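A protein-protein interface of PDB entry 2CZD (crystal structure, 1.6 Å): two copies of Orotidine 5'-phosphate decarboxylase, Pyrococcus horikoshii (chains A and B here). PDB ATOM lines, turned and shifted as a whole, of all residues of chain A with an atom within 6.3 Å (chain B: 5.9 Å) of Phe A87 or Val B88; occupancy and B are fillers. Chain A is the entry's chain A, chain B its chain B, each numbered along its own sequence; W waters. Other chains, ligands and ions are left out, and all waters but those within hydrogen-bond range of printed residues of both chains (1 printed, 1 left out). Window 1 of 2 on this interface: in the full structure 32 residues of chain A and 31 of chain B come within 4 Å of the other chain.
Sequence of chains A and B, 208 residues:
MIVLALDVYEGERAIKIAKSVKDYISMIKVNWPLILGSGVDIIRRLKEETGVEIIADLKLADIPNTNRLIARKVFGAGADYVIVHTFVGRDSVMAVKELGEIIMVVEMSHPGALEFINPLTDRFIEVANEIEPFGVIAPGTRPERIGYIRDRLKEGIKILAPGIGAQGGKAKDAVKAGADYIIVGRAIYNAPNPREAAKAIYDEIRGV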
ATOM      1  N   ALA A  61      -6.620   1.659  12.228  1.00  0.00           N
ATOM      2  CA  ALA A  61      -5.716   2.509  12.992  1.00  0.00           C
ATOM      3  C   ALA A  61      -4.327   1.926  12.989  1.00  0.00           C
ATOM      4  O   ALA A  61      -3.652   1.886  14.021  1.00  0.00           O
ATOM      5  CB  ALA A  61      -6.239   2.636  14.436  1.00  0.00           C
ATOM      6  N   HIS A  85      -9.872   5.612  11.493  1.00  0.00           N
ATOM      7  CA  HIS A  85      -9.568   6.617  12.507  1.00  0.00           C
ATOM      8  C   HIS A  85      -8.716   7.736  11.926  1.00  0.00           C
ATOM      9  O   HIS A  85      -7.939   7.539  10.994  1.00  0.00           O
ATOM     10  CB  HIS A  85      -8.784   6.007  13.668  1.00  0.00           C
ATOM     11  CG  HIS A  85      -9.641   5.483  14.772  1.00  0.00           C
ATOM     12  ND1 HIS A  85     -10.391   6.310  15.579  1.00  0.00           N
ATOM     13  CD2 HIS A  85      -9.839   4.221  15.229  1.00  0.00           C
ATOM     14  CE1 HIS A  85     -11.018   5.583  16.486  1.00  0.00           C
ATOM     15  NE2 HIS A  85     -10.701   4.310  16.299  1.00  0.00           N
ATOM     16  N   THR A  86      -8.873   8.909  12.506  1.00  0.00           N
ATOM     17  CA  THR A  86      -8.100  10.065  12.108  1.00  0.00           C
ATOM     18  C   THR A  86      -6.824  10.141  12.941  1.00  0.00           C
ATOM     19  O   THR A  86      -5.781  10.594  12.448  1.00  0.00           O
ATOM     20  CB  THR A  86      -8.908  11.335  12.386  1.00  0.00           C
ATOM     21  OG1 THR A  86     -10.156  11.261  11.698  1.00  0.00           O
ATOM     22  CG2 THR A  86      -8.164  12.562  11.901  1.00  0.00           C
ATOM     23  N   PHE A  87      -6.881   9.642  14.176  1.00  0.00           N
ATOM     24  CA  PHE A  87      -5.744   9.821  15.087  1.00  0.00           C
ATOM     25  C   PHE A  87      -4.411   9.237  14.691  1.00  0.00           C
ATOM     26  O   PHE A  87      -3.375   9.723  15.142  1.00  0.00           O
ATOM     27  CB  PHE A  87      -6.131   9.395  16.522  1.00  0.00           C
ATOM     28  CG  PHE A  87      -6.125   7.926  16.773  1.00  0.00           C
ATOM     29  CD1 PHE A  87      -4.925   7.228  16.914  1.00  0.00           C
ATOM     30  CD2 PHE A  87      -7.315   7.246  16.993  1.00  0.00           C
ATOM     31  CE1 PHE A  87      -4.931   5.873  17.284  1.00  0.00           C
ATOM     32  CE2 PHE A  87      -7.322   5.886  17.366  1.00  0.00           C
ATOM     33  CZ  PHE A  87      -6.137   5.209  17.514  1.00  0.00           C
ATOM     34  N   VAL A  88      -4.419   8.224  13.834  1.00  0.00           N
ATOM     35  CA  VAL A  88      -3.153   7.619  13.434  1.00  0.00           C
ATOM     36  C   VAL A  88      -2.405   8.440  12.379  1.00  0.00           C
ATOM     37  O   VAL A  88      -1.267   8.131  12.042  1.00  0.00           O
ATOM     38  CB  VAL A  88      -3.381   6.137  13.005  1.00  0.00           C
ATOM     39  CG1 VAL A  88      -2.090   5.465  12.551  1.00  0.00           C
ATOM     40  CG2 VAL A  88      -3.908   5.369  14.197  1.00  0.00           C
ATOM     41  N   GLY A  89      -3.030   9.492  11.868  1.00  0.00           N
ATOM     42  CA  GLY A  89      -2.328  10.340  10.921  1.00  0.00           C
ATOM     43  C   GLY A  89      -2.847  10.325   9.508  1.00  0.00           C
ATOM     44  O   GLY A  89      -3.513   9.377   9.091  1.00  0.00           O
ATOM     45  N   VAL A  93      -4.636   7.399   6.760  1.00  0.00           N
ATOM     46  CA  VAL A  93      -5.968   7.642   6.205  1.00  0.00           C
ATOM     47  C   VAL A  93      -5.906   7.582   4.675  1.00  0.00           C
ATOM     48  O   VAL A  93      -6.738   6.915   4.044  1.00  0.00           O
ATOM     49  CB  VAL A  93      -6.531   9.037   6.625  1.00  0.00           C
ATOM     50  CG1 VAL A  93      -7.879   9.302   5.951  1.00  0.00           C
ATOM     51  CG2 VAL A  93      -6.744   9.090   8.143  1.00  0.00           C
ATOM     52  N   VAL A 105     -13.407   8.874  11.657  1.00  0.00           N
ATOM     53  CA  VAL A 105     -13.853   9.004  13.051  1.00  0.00           C
ATOM     54  C   VAL A 105     -13.201  10.251  13.622  1.00  0.00           C
ATOM     55  O   VAL A 105     -11.970  10.358  13.648  1.00  0.00           O
ATOM     56  CB  VAL A 105     -13.401   7.784  13.895  1.00  0.00           C
ATOM     57  CG1 VAL A 105     -13.778   7.987  15.372  1.00  0.00           C
ATOM     58  CG2 VAL A 105     -14.066   6.533  13.368  1.00  0.00           C
ATOM     59  N   MET A 108     -15.970  10.217  19.583  1.00  0.00           N
ATOM     60  CA  MET A 108     -16.624   8.984  20.002  1.00  0.00           C
ATOM     61  C   MET A 108     -17.518   9.274  21.212  1.00  0.00           C
ATOM     62  O   MET A 108     -17.481  10.375  21.763  1.00  0.00           O
ATOM     63  CB  MET A 108     -15.592   7.894  20.267  1.00  0.00           C
ATOM     64  CG  MET A 108     -14.925   7.447  18.966  1.00  0.00           C
ATOM     65  SD  MET A 108     -13.647   6.208  19.165  1.00  0.00           S
ATOM     66  CE  MET A 108     -14.594   4.725  19.132  1.00  0.00           C
ATOM     67  N   HIS A 110     -18.249   6.833  24.041  1.00  0.00           N
ATOM     68  CA  HIS A 110     -18.075   6.047  25.259  1.00  0.00           C
ATOM     69  C   HIS A 110     -17.259   6.915  26.216  1.00  0.00           C
ATOM     70  O   HIS A 110     -16.549   7.831  25.795  1.00  0.00           O
ATOM     71  CB  HIS A 110     -17.345   4.738  24.950  1.00  0.00           C
ATOM     72  CG  HIS A 110     -16.009   4.932  24.301  1.00  0.00           C
ATOM     73  ND1 HIS A 110     -15.868   5.373  23.000  1.00  0.00           N
ATOM     74  CD2 HIS A 110     -14.757   4.716  24.767  1.00  0.00           C
ATOM     75  CE1 HIS A 110     -14.582   5.419  22.695  1.00  0.00           C
ATOM     76  NE2 HIS A 110     -13.888   5.027  23.750  1.00  0.00           N
ATOM     77  N   PRO A 111     -17.326   6.631  27.533  1.00  0.00           N
ATOM     78  CA  PRO A 111     -16.580   7.422  28.508  1.00  0.00           C
ATOM     79  C   PRO A 111     -15.106   7.598  28.191  1.00  0.00           C
ATOM     80  O   PRO A 111     -14.542   8.683  28.336  1.00  0.00           O
ATOM     81  CB  PRO A 111     -16.826   6.683  29.826  1.00  0.00           C
ATOM     82  CG  PRO A 111     -18.201   6.088  29.630  1.00  0.00           C
ATOM     83  CD  PRO A 111     -18.189   5.624  28.177  1.00  0.00           C
ATOM     84  N   GLY A 112     -14.479   6.517  27.750  1.00  0.00           N
ATOM     85  CA  GLY A 112     -13.070   6.584  27.421  1.00  0.00           C
ATOM     86  C   GLY A 112     -12.695   7.597  26.346  1.00  0.00           C
ATOM     87  O   GLY A 112     -11.542   8.024  26.277  1.00  0.00           O
ATOM     88  N   ALA A 113     -13.657   7.977  25.504  1.00  0.00           N
ATOM     89  CA  ALA A 113     -13.396   8.945  24.437  1.00  0.00           C
ATOM     90  C   ALA A 113     -13.020  10.327  24.997  1.00  0.00           C
ATOM     91  O   ALA A 113     -12.390  11.131  24.311  1.00  0.00           O
ATOM     92  CB  ALA A 113     -14.622   9.070  23.538  1.00  0.00           C
ATOM     93  N   LEU A 114     -13.377  10.587  26.248  1.00  0.00           N
ATOM     94  CA  LEU A 114     -13.048  11.885  26.849  1.00  0.00           C
ATOM     95  C   LEU A 114     -11.567  12.032  27.175  1.00  0.00           C
ATOM     96  O   LEU A 114     -11.062  13.148  27.349  1.00  0.00           O
ATOM     97  CB  LEU A 114     -13.854  12.080  28.139  1.00  0.00           C
ATOM     98  CG  LEU A 114     -15.369  12.090  27.994  1.00  0.00           C
ATOM     99  CD1 LEU A 114     -15.989  12.194  29.385  1.00  0.00           C
ATOM    100  CD2 LEU A 114     -15.795  13.270  27.134  1.00  0.00           C
ATOM    101  N   GLU A 115     -10.850  10.914  27.223  1.00  0.00           N
ATOM    102  CA  GLU A 115      -9.441  10.950  27.591  1.00  0.00           C
ATOM    103  C   GLU A 115      -8.522  11.594  26.549  1.00  0.00           C
ATOM    104  O   GLU A 115      -7.750  12.517  26.862  1.00  0.00           O
ATOM    105  CB  GLU A 115      -8.952   9.523  27.884  1.00  0.00           C
ATOM    106  CG  GLU A 115      -9.606   8.820  29.061  1.00  0.00           C
ATOM    107  CD  GLU A 115      -9.146   7.360  29.131  1.00  0.00           C
ATOM    108  OE1 GLU A 115      -7.984   7.091  28.781  1.00  0.00           O
ATOM    109  OE2 GLU A 115      -9.934   6.506  29.532  1.00  0.00           O
ATOM    110  N   PHE A 116      -8.631  11.137  25.301  1.00  0.00           N
ATOM    111  CA  PHE A 116      -7.764  11.613  24.243  1.00  0.00           C
ATOM    112  C   PHE A 116      -8.439  11.974  22.933  1.00  0.00           C
ATOM    113  O   PHE A 116      -8.045  12.929  22.280  1.00  0.00           O
ATOM    114  CB  PHE A 116      -6.687  10.555  23.929  1.00  0.00           C
ATOM    115  CG  PHE A 116      -5.857  10.153  25.123  1.00  0.00           C
ATOM    116  CD1 PHE A 116      -6.066   8.931  25.742  1.00  0.00           C
ATOM    117  CD2 PHE A 116      -4.876  11.005  25.623  1.00  0.00           C
ATOM    118  CE1 PHE A 116      -5.310   8.551  26.849  1.00  0.00           C
ATOM    119  CE2 PHE A 116      -4.116  10.642  26.729  1.00  0.00           C
ATOM    120  CZ  PHE A 116      -4.336   9.408  27.342  1.00  0.00           C
ATOM    121  N   ILE A 117      -9.449  11.208  22.545  1.00  0.00           N
ATOM    122  CA  ILE A 117     -10.106  11.453  21.272  1.00  0.00           C
ATOM    123  C   ILE A 117     -10.910  12.746  21.220  1.00  0.00           C
ATOM    124  O   ILE A 117     -10.649  13.622  20.389  1.00  0.00           O
ATOM    125  CB  ILE A 117     -11.042  10.270  20.884  1.00  0.00           C
ATOM    126  CG1 ILE A 117     -10.211   9.015  20.622  1.00  0.00           C
ATOM    127  CG2 ILE A 117     -11.878  10.628  19.650  1.00  0.00           C
ATOM    128  CD1 ILE A 117     -11.063   7.819  20.277  1.00  0.00           C
ATOM    129  N   LEU A 120      -9.500  16.219  20.886  1.00  0.00           N
ATOM    130  CA  LEU A 120      -8.922  16.506  19.577  1.00  0.00           C
ATOM    131  C   LEU A 120      -9.953  16.584  18.461  1.00  0.00           C
ATOM    132  O   LEU A 120      -9.585  16.735  17.300  1.00  0.00           O
ATOM    133  CB  LEU A 120      -7.851  15.446  19.228  1.00  0.00           C
ATOM    134  CG  LEU A 120      -6.503  15.583  19.938  1.00  0.00           C
ATOM    135  CD1 LEU A 120      -5.707  14.289  19.785  1.00  0.00           C
ATOM    136  CD2 LEU A 120      -5.717  16.772  19.327  1.00  0.00           C
ATOM    137  N   PHE A 124      -9.380  17.009  14.477  1.00  0.00           N
ATOM    138  CA  PHE A 124      -9.691  15.912  13.569  1.00  0.00           C
ATOM    139  C   PHE A 124     -10.643  16.373  12.473  1.00  0.00           C
ATOM    140  O   PHE A 124     -10.551  15.892  11.339  1.00  0.00           O
ATOM    141  CB  PHE A 124     -10.309  14.724  14.325  1.00  0.00           C
ATOM    142  CG  PHE A 124      -9.356  14.029  15.269  1.00  0.00           C
ATOM    143  CD1 PHE A 124      -7.984  14.016  15.031  1.00  0.00           C
ATOM    144  CD2 PHE A 124      -9.860  13.307  16.353  1.00  0.00           C
ATOM    145  CE1 PHE A 124      -7.118  13.283  15.865  1.00  0.00           C
ATOM    146  CE2 PHE A 124      -9.009  12.577  17.183  1.00  0.00           C
ATOM    147  CZ  PHE A 124      -7.641  12.565  16.938  1.00  0.00           C
ATOM    148  N   LEU B  60      -6.484  -2.867  18.257  1.00  0.00           N
ATOM    149  CA  LEU B  60      -7.908  -2.600  18.473  1.00  0.00           C
ATOM    150  C   LEU B  60      -8.122  -1.165  18.934  1.00  0.00           C
ATOM    151  O   LEU B  60      -7.409  -0.657  19.817  1.00  0.00           O
ATOM    152  CB  LEU B  60      -8.520  -3.576  19.478  1.00  0.00           C
ATOM    153  CG  LEU B  60      -8.581  -5.047  19.017  1.00  0.00           C
ATOM    154  CD1 LEU B  60      -9.295  -5.862  20.116  1.00  0.00           C
ATOM    155  CD2 LEU B  60      -9.275  -5.182  17.651  1.00  0.00           C
ATOM    156  N   ALA B  61      -9.124  -0.533  18.328  1.00  0.00           N
ATOM    157  CA  ALA B  61      -9.424   0.874  18.584  1.00  0.00           C
ATOM    158  C   ALA B  61     -10.931   1.126  18.478  1.00  0.00           C
ATOM    159  O   ALA B  61     -11.385   2.167  17.991  1.00  0.00           O
ATOM    160  CB  ALA B  61      -8.674   1.726  17.555  1.00  0.00           C
ATOM    161  N   ASP B  62     -11.717   0.158  18.911  1.00  0.00           N
ATOM    162  CA  ASP B  62     -13.159   0.333  18.838  1.00  0.00           C
ATOM    163  C   ASP B  62     -13.765   0.648  20.212  1.00  0.00           C
ATOM    164  O   ASP B  62     -13.043   0.830  21.221  1.00  0.00           O
ATOM    165  CB  ASP B  62     -13.797  -0.941  18.259  1.00  0.00           C
ATOM    166  CG  ASP B  62     -14.934  -0.630  17.297  1.00  0.00           C
ATOM    167  OD1 ASP B  62     -15.888   0.056  17.706  1.00  0.00           O
ATOM    168  OD2 ASP B  62     -14.881  -1.071  16.132  1.00  0.00           O
ATOM    169  N   ILE B  63     -15.098   0.742  20.251  1.00  0.00           N
ATOM    170  CA  ILE B  63     -15.785   0.982  21.511  1.00  0.00           C
ATOM    171  C   ILE B  63     -15.586  -0.255  22.397  1.00  0.00           C
ATOM    172  O   ILE B  63     -15.327  -1.368  21.907  1.00  0.00           O
ATOM    173  CB  ILE B  63     -17.289   1.269  21.298  1.00  0.00           C
ATOM    174  CG1 ILE B  63     -18.017   0.031  20.790  1.00  0.00           C
ATOM    175  CG2 ILE B  63     -17.437   2.392  20.295  1.00  0.00           C
ATOM    176  CD1 ILE B  63     -19.536   0.264  20.620  1.00  0.00           C
ATOM    177  N   ASN B  67     -14.647  -4.072  21.109  1.00  0.00           N
ATOM    178  CA  ASN B  67     -13.307  -4.569  21.409  1.00  0.00           C
ATOM    179  C   ASN B  67     -13.452  -5.906  22.133  1.00  0.00           C
ATOM    180  O   ASN B  67     -12.726  -6.862  21.854  1.00  0.00           O
ATOM    181  CB  ASN B  67     -12.565  -3.599  22.334  1.00  0.00           C
ATOM    182  CG  ASN B  67     -11.716  -2.603  21.572  1.00  0.00           C
ATOM    183  OD1 ASN B  67     -11.871  -2.438  20.362  1.00  0.00           O
ATOM    184  ND2 ASN B  67     -10.812  -1.928  22.284  1.00  0.00           N
ATOM    185  N   HIS B  85      -4.787  -0.330  21.074  1.00  0.00           N
ATOM    186  CA  HIS B  85      -4.380   1.078  21.166  1.00  0.00           C
ATOM    187  C   HIS B  85      -4.748   1.614  22.544  1.00  0.00           C
ATOM    188  O   HIS B  85      -5.637   1.086  23.216  1.00  0.00           O
ATOM    189  CB  HIS B  85      -5.124   1.938  20.138  1.00  0.00           C
ATOM    190  CG  HIS B  85      -4.387   2.120  18.849  1.00  0.00           C
ATOM    191  ND1 HIS B  85      -3.238   2.874  18.749  1.00  0.00           N
ATOM    192  CD2 HIS B  85      -4.649   1.656  17.599  1.00  0.00           C
ATOM    193  CE1 HIS B  85      -2.821   2.870  17.494  1.00  0.00           C
ATOM    194  NE2 HIS B  85      -3.661   2.137  16.774  1.00  0.00           N
ATOM    195  N   THR B  86      -4.039   2.667  22.936  1.00  0.00           N
ATOM    196  CA  THR B  86      -4.270   3.366  24.196  1.00  0.00           C
ATOM    197  C   THR B  86      -5.194   4.568  23.956  1.00  0.00           C
ATOM    198  O   THR B  86      -5.966   4.944  24.838  1.00  0.00           O
ATOM    199  CB  THR B  86      -2.940   3.922  24.765  1.00  0.00           C
ATOM    200  OG1 THR B  86      -2.021   2.838  24.923  1.00  0.00           O
ATOM    201  CG2 THR B  86      -3.136   4.558  26.130  1.00  0.00           C
ATOM    202  N   PHE B  87      -5.103   5.151  22.753  1.00  0.00           N
ATOM    203  CA  PHE B  87      -5.817   6.392  22.367  1.00  0.00           C
ATOM    204  C   PHE B  87      -7.321   6.419  22.592  1.00  0.00           C
ATOM    205  O   PHE B  87      -7.873   7.455  22.947  1.00  0.00           O
ATOM    206  CB  PHE B  87      -5.530   6.683  20.867  1.00  0.00           C
ATOM    207  CG  PHE B  87      -5.302   8.140  20.508  1.00  0.00           C
ATOM    208  CD1 PHE B  87      -6.289   9.096  20.697  1.00  0.00           C
ATOM    209  CD2 PHE B  87      -4.104   8.536  19.914  1.00  0.00           C
ATOM    210  CE1 PHE B  87      -6.079  10.444  20.301  1.00  0.00           C
ATOM    211  CE2 PHE B  87      -3.897   9.896  19.515  1.00  0.00           C
ATOM    212  CZ  PHE B  87      -4.887  10.822  19.720  1.00  0.00           C
ATOM    213  N   VAL B  88      -7.979   5.281  22.403  1.00  0.00           N
ATOM    214  CA  VAL B  88      -9.422   5.210  22.500  1.00  0.00           C
ATOM    215  C   VAL B  88      -9.960   5.212  23.924  1.00  0.00           C
ATOM    216  O   VAL B  88     -11.154   5.375  24.133  1.00  0.00           O
ATOM    217  CB  VAL B  88      -9.921   3.993  21.655  1.00  0.00           C
ATOM    218  CG1 VAL B  88     -11.437   3.867  21.668  1.00  0.00           C
ATOM    219  CG2 VAL B  88      -9.471   4.204  20.201  1.00  0.00           C
ATOM    220  N   GLY B  89      -9.084   5.040  24.906  1.00  0.00           N
ATOM    221  CA  GLY B  89      -9.562   5.089  26.275  1.00  0.00           C
ATOM    222  C   GLY B  89      -9.285   3.839  27.081  1.00  0.00           C
ATOM    223  O   GLY B  89      -9.110   2.758  26.528  1.00  0.00           O
ATOM    224  N   ARG B  90      -9.258   4.006  28.399  1.00  0.00           N
ATOM    225  CA  ARG B  90      -9.004   2.906  29.322  1.00  0.00           C
ATOM    226  C   ARG B  90     -10.112   1.841  29.301  1.00  0.00           C
ATOM    227  O   ARG B  90      -9.829   0.659  29.487  1.00  0.00           O
ATOM    228  CB  ARG B  90      -8.851   3.464  30.736  1.00  0.00           C
ATOM    229  CG  ARG B  90      -7.626   4.353  30.882  1.00  0.00           C
ATOM    230  CD  ARG B  90      -7.725   5.175  32.170  1.00  0.00           C
ATOM    231  NE  ARG B  90      -6.511   5.932  32.515  1.00  0.00           N
ATOM    232  CZ  ARG B  90      -6.083   7.060  31.937  1.00  0.00           C
ATOM    233  NH1 ARG B  90      -6.743   7.631  30.928  1.00  0.00           N
ATOM    234  NH2 ARG B  90      -4.987   7.656  32.417  1.00  0.00           N
ATOM    235  N   ASP B  91     -11.359   2.247  29.077  1.00  0.00           N
ATOM    236  CA  ASP B  91     -12.439   1.271  29.021  1.00  0.00           C
ATOM    237  C   ASP B  91     -12.267   0.336  27.832  1.00  0.00           C
ATOM    238  O   ASP B  91     -12.476  -0.872  27.962  1.00  0.00           O
ATOM    239  CB  ASP B  91     -13.839   1.934  29.039  1.00  0.00           C
ATOM    240  CG  ASP B  91     -13.986   3.097  28.063  1.00  0.00           C
ATOM    241  OD1 ASP B  91     -15.068   3.727  28.078  1.00  0.00           O
ATOM    242  OD2 ASP B  91     -13.061   3.391  27.295  1.00  0.00           O
ATOM    243  N   SER B  92     -11.878   0.884  26.683  1.00  0.00           N
ATOM    244  CA  SER B  92     -11.644   0.052  25.515  1.00  0.00           C
ATOM    245  C   SER B  92     -10.451  -0.882  25.728  1.00  0.00           C
ATOM    246  O   SER B  92     -10.468  -2.014  25.240  1.00  0.00           O
ATOM    247  CB  SER B  92     -11.464   0.911  24.263  1.00  0.00           C
ATOM    248  OG  SER B  92     -12.723   1.460  23.879  1.00  0.00           O
ATOM    249  N   MET B 108       4.127   5.095  17.638  1.00  0.00           N
ATOM    250  CA  MET B 108       4.146   4.399  16.355  1.00  0.00           C
ATOM    251  C   MET B 108       5.318   4.800  15.470  1.00  0.00           C
ATOM    252  O   MET B 108       5.963   5.829  15.700  1.00  0.00           O
ATOM    253  CB  MET B 108       2.801   4.550  15.650  1.00  0.00           C
ATOM    254  CG  MET B 108       1.786   3.629  16.292  1.00  0.00           C
ATOM    255  SD  MET B 108       0.151   3.724  15.542  1.00  0.00           S
ATOM    256  CE  MET B 108       0.342   2.561  14.174  1.00  0.00           C
ATOM    257  N   GLY B 112       2.968   9.484   9.902  1.00  0.00           N
ATOM    258  CA  GLY B 112       1.741  10.004  10.480  1.00  0.00           C
ATOM    259  C   GLY B 112       1.704   9.960  11.999  1.00  0.00           C
ATOM    260  O   GLY B 112       0.913  10.698  12.631  1.00  0.00           O
ATOM    261  N   GLU B 115       1.869  13.190  14.104  1.00  0.00           N
ATOM    262  CA  GLU B 115       0.775  14.130  14.160  1.00  0.00           C
ATOM    263  C   GLU B 115      -0.034  14.153  15.459  1.00  0.00           C
ATOM    264  O   GLU B 115      -0.311  15.236  15.986  1.00  0.00           O
ATOM    265  CB  GLU B 115      -0.136  13.909  12.946  1.00  0.00           C
ATOM    266  CG  GLU B 115       0.595  14.260  11.650  1.00  0.00           C
ATOM    267  CD  GLU B 115      -0.127  13.834  10.378  1.00  0.00           C
ATOM    268  OE1 GLU B 115      -1.319  13.457  10.430  1.00  0.00           O
ATOM    269  OE2 GLU B 115       0.516  13.910   9.312  1.00  0.00           O
ATOM    270  N   PHE B 116      -0.406  12.979  15.969  1.00  0.00           N
ATOM    271  CA  PHE B 116      -1.202  12.916  17.191  1.00  0.00           C
ATOM    272  C   PHE B 116      -0.736  11.884  18.211  1.00  0.00           C
ATOM    273  O   PHE B 116      -0.763  12.142  19.406  1.00  0.00           O
ATOM    274  CB  PHE B 116      -2.678  12.612  16.862  1.00  0.00           C
ATOM    275  CG  PHE B 116      -3.313  13.597  15.925  1.00  0.00           C
ATOM    276  CD1 PHE B 116      -3.534  13.274  14.583  1.00  0.00           C
ATOM    277  CD2 PHE B 116      -3.698  14.856  16.385  1.00  0.00           C
ATOM    278  CE1 PHE B 116      -4.138  14.198  13.704  1.00  0.00           C
ATOM    279  CE2 PHE B 116      -4.304  15.786  15.515  1.00  0.00           C
ATOM    280  CZ  PHE B 116      -4.522  15.452  14.177  1.00  0.00           C
ATOM    281  N   ILE B 117      -0.342  10.707  17.744  1.00  0.00           N
ATOM    282  CA  ILE B 117       0.076   9.643  18.639  1.00  0.00           C
ATOM    283  C   ILE B 117       1.374   9.928  19.394  1.00  0.00           C
ATOM    284  O   ILE B 117       1.392   9.976  20.619  1.00  0.00           O
ATOM    285  CB  ILE B 117       0.253   8.317  17.855  1.00  0.00           C
ATOM    286  CG1 ILE B 117      -1.096   7.840  17.303  1.00  0.00           C
ATOM    287  CG2 ILE B 117       0.873   7.261  18.746  1.00  0.00           C
ATOM    288  CD1 ILE B 117      -1.961   7.096  18.291  1.00  0.00           C
HETATM  289  O   HOH W   1      -0.718  10.338  14.826  1.00  0.00           O
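Of the 19 printed residues of chain A, 15 touch a printed residue of chain B.
Hydrophobic or aromatic side chains of chain A within 4 Å of the printed part of chain B: Ala A61, His A85, Phe A87, Met A108, His A110, Pro A111, Phe A116, Ile A117, Leu A120 and Phe A124.
Hydrophobic or aromatic side chains of chain B that line the printed part of chain A: Ala B61, Ile B63, His B85, Phe B87, Val B88, Phe B116 and Ile B117.
Among the printed residues, 27 pairs touch across the chains.
Among the printed residues, Asp or Glu carboxylates within 4 Å of a Lys or Arg side-chain nitrogen of the other chain: Glu A115 with Arg B90 (2.5 Å).
The backbone carbonyl oxygen of Gly A112 lies close to the backbone carbonyl oxygen of Val B88 (3.4 Å).
NH1 of Arg B90 lies within salt-bridge range of OE1 of Glu A115, 2.5 Å away.
O of Ala B61 lies within hydrogen-bond range of NE2 of His A85, at 2.8 Å.
O of Val A88 lies close to O of Gly B112 (3.4 Å).
O of Val B88 lies within hydrogen-bond range of NE2 of His A110, at 2.8 Å.
The backbone carbonyl oxygen of Ala A61 lies within hydrogen-bond range of a ring nitrogen (NE2) of His B85 (2.8 Å).
N of Gly A112 sits at hydrogen-bond distance from OD1 of Asp B91 (2.9 Å).
The side-chain amide nitrogen (ND2) of Asn B67 lies within hydrogen-bond range of the backbone carbonyl oxygen (O) of Ser B92 (3.0 Å).
The backbone NH (N) of Ala A113 lies within hydrogen-bond range of a ring nitrogen (NE2) of His A110 (3.4 Å).
The backbone carbonyl oxygen (O) of Asp B62 lies within hydrogen-bond range of the side-chain hydroxyl (OG) of Ser B92, at 2.8 Å.
The backbone carbonyl oxygen (O) of Leu B60 lies within hydrogen-bond range of the backbone NH (N) of His B85, 2.9 Å away.
CE1 of Phe A87 touches CE1 of His B85, at 3.7 Å.
CE2 of Phe A87 touches CG2 of Val B88, at 3.9 Å.
Gly B112 touches Gly A89 (O to CA, 3.7 Å).
Asp B91 touches His A110.
Asp B91 touches Pro A111 (OD1 to CD, 3.7 Å).
OE2 of Glu A115 touches CA of Gly B89, 3.6 Å away.
Phe A116 touches Phe B87 (CB to O, 3.5 Å).
Ile A117 touches Phe B87 (CG1 to O, 3.6 Å).
Ile A117 touches Val B88.
Phe A124 touches Phe B116.
Printed residues of chain B within 4 Å of His A85: Ala B61.
Val A105 touches none of the printed residues of chain B.
Leu A114 touches none of the printed residues of chain B.
Printed residues of chain A within 4 Å of His B85: Ala A61 (2.8 Å) and Phe A87 (3.7 Å).
Of chain A, only Phe A87, His A110, Gly A112, Ala A113 and Ile A117 come within 4 Å of Val B88.
Of the printed residues of chain A, Glu B115 touches Gly A89.
Of the printed residues of chain A, Ile B117 touches Phe A87.
Phe A87 touches Val B88, but with the chains exchanged Val A88 does not touch Phe B87 (5.9 Å).
Phe A87 touches Ile B117, and with the chains exchanged Ile A117 touches Phe B87.
Gly A89 touches Gly B112, and with the chains exchanged Gly A112 touches Gly B89.
Ile A117 touches Val B88, but with the chains exchanged Val A88 does not touch Ile B117 (4.4 Å).
Positions printed for both chains: 61, 85, 86, 87, 88, 89, 108, 112, 115, 116 and 117.
Of the 27 pairs that touch across the chains among the printed residues, 13 have their exchanged pair printed and touching as well.
Water W1 lies within hydrogen-bond range of the backbone carbonyl oxygen (O) of Phe A87 (2.7 Å), the backbone carbonyl oxygen (O) of Gly B112 (2.8 Å), the backbone NH (N) of Phe B116 (2.9 Å) and the backbone NH (N) of Ile B117 (3.0 Å).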
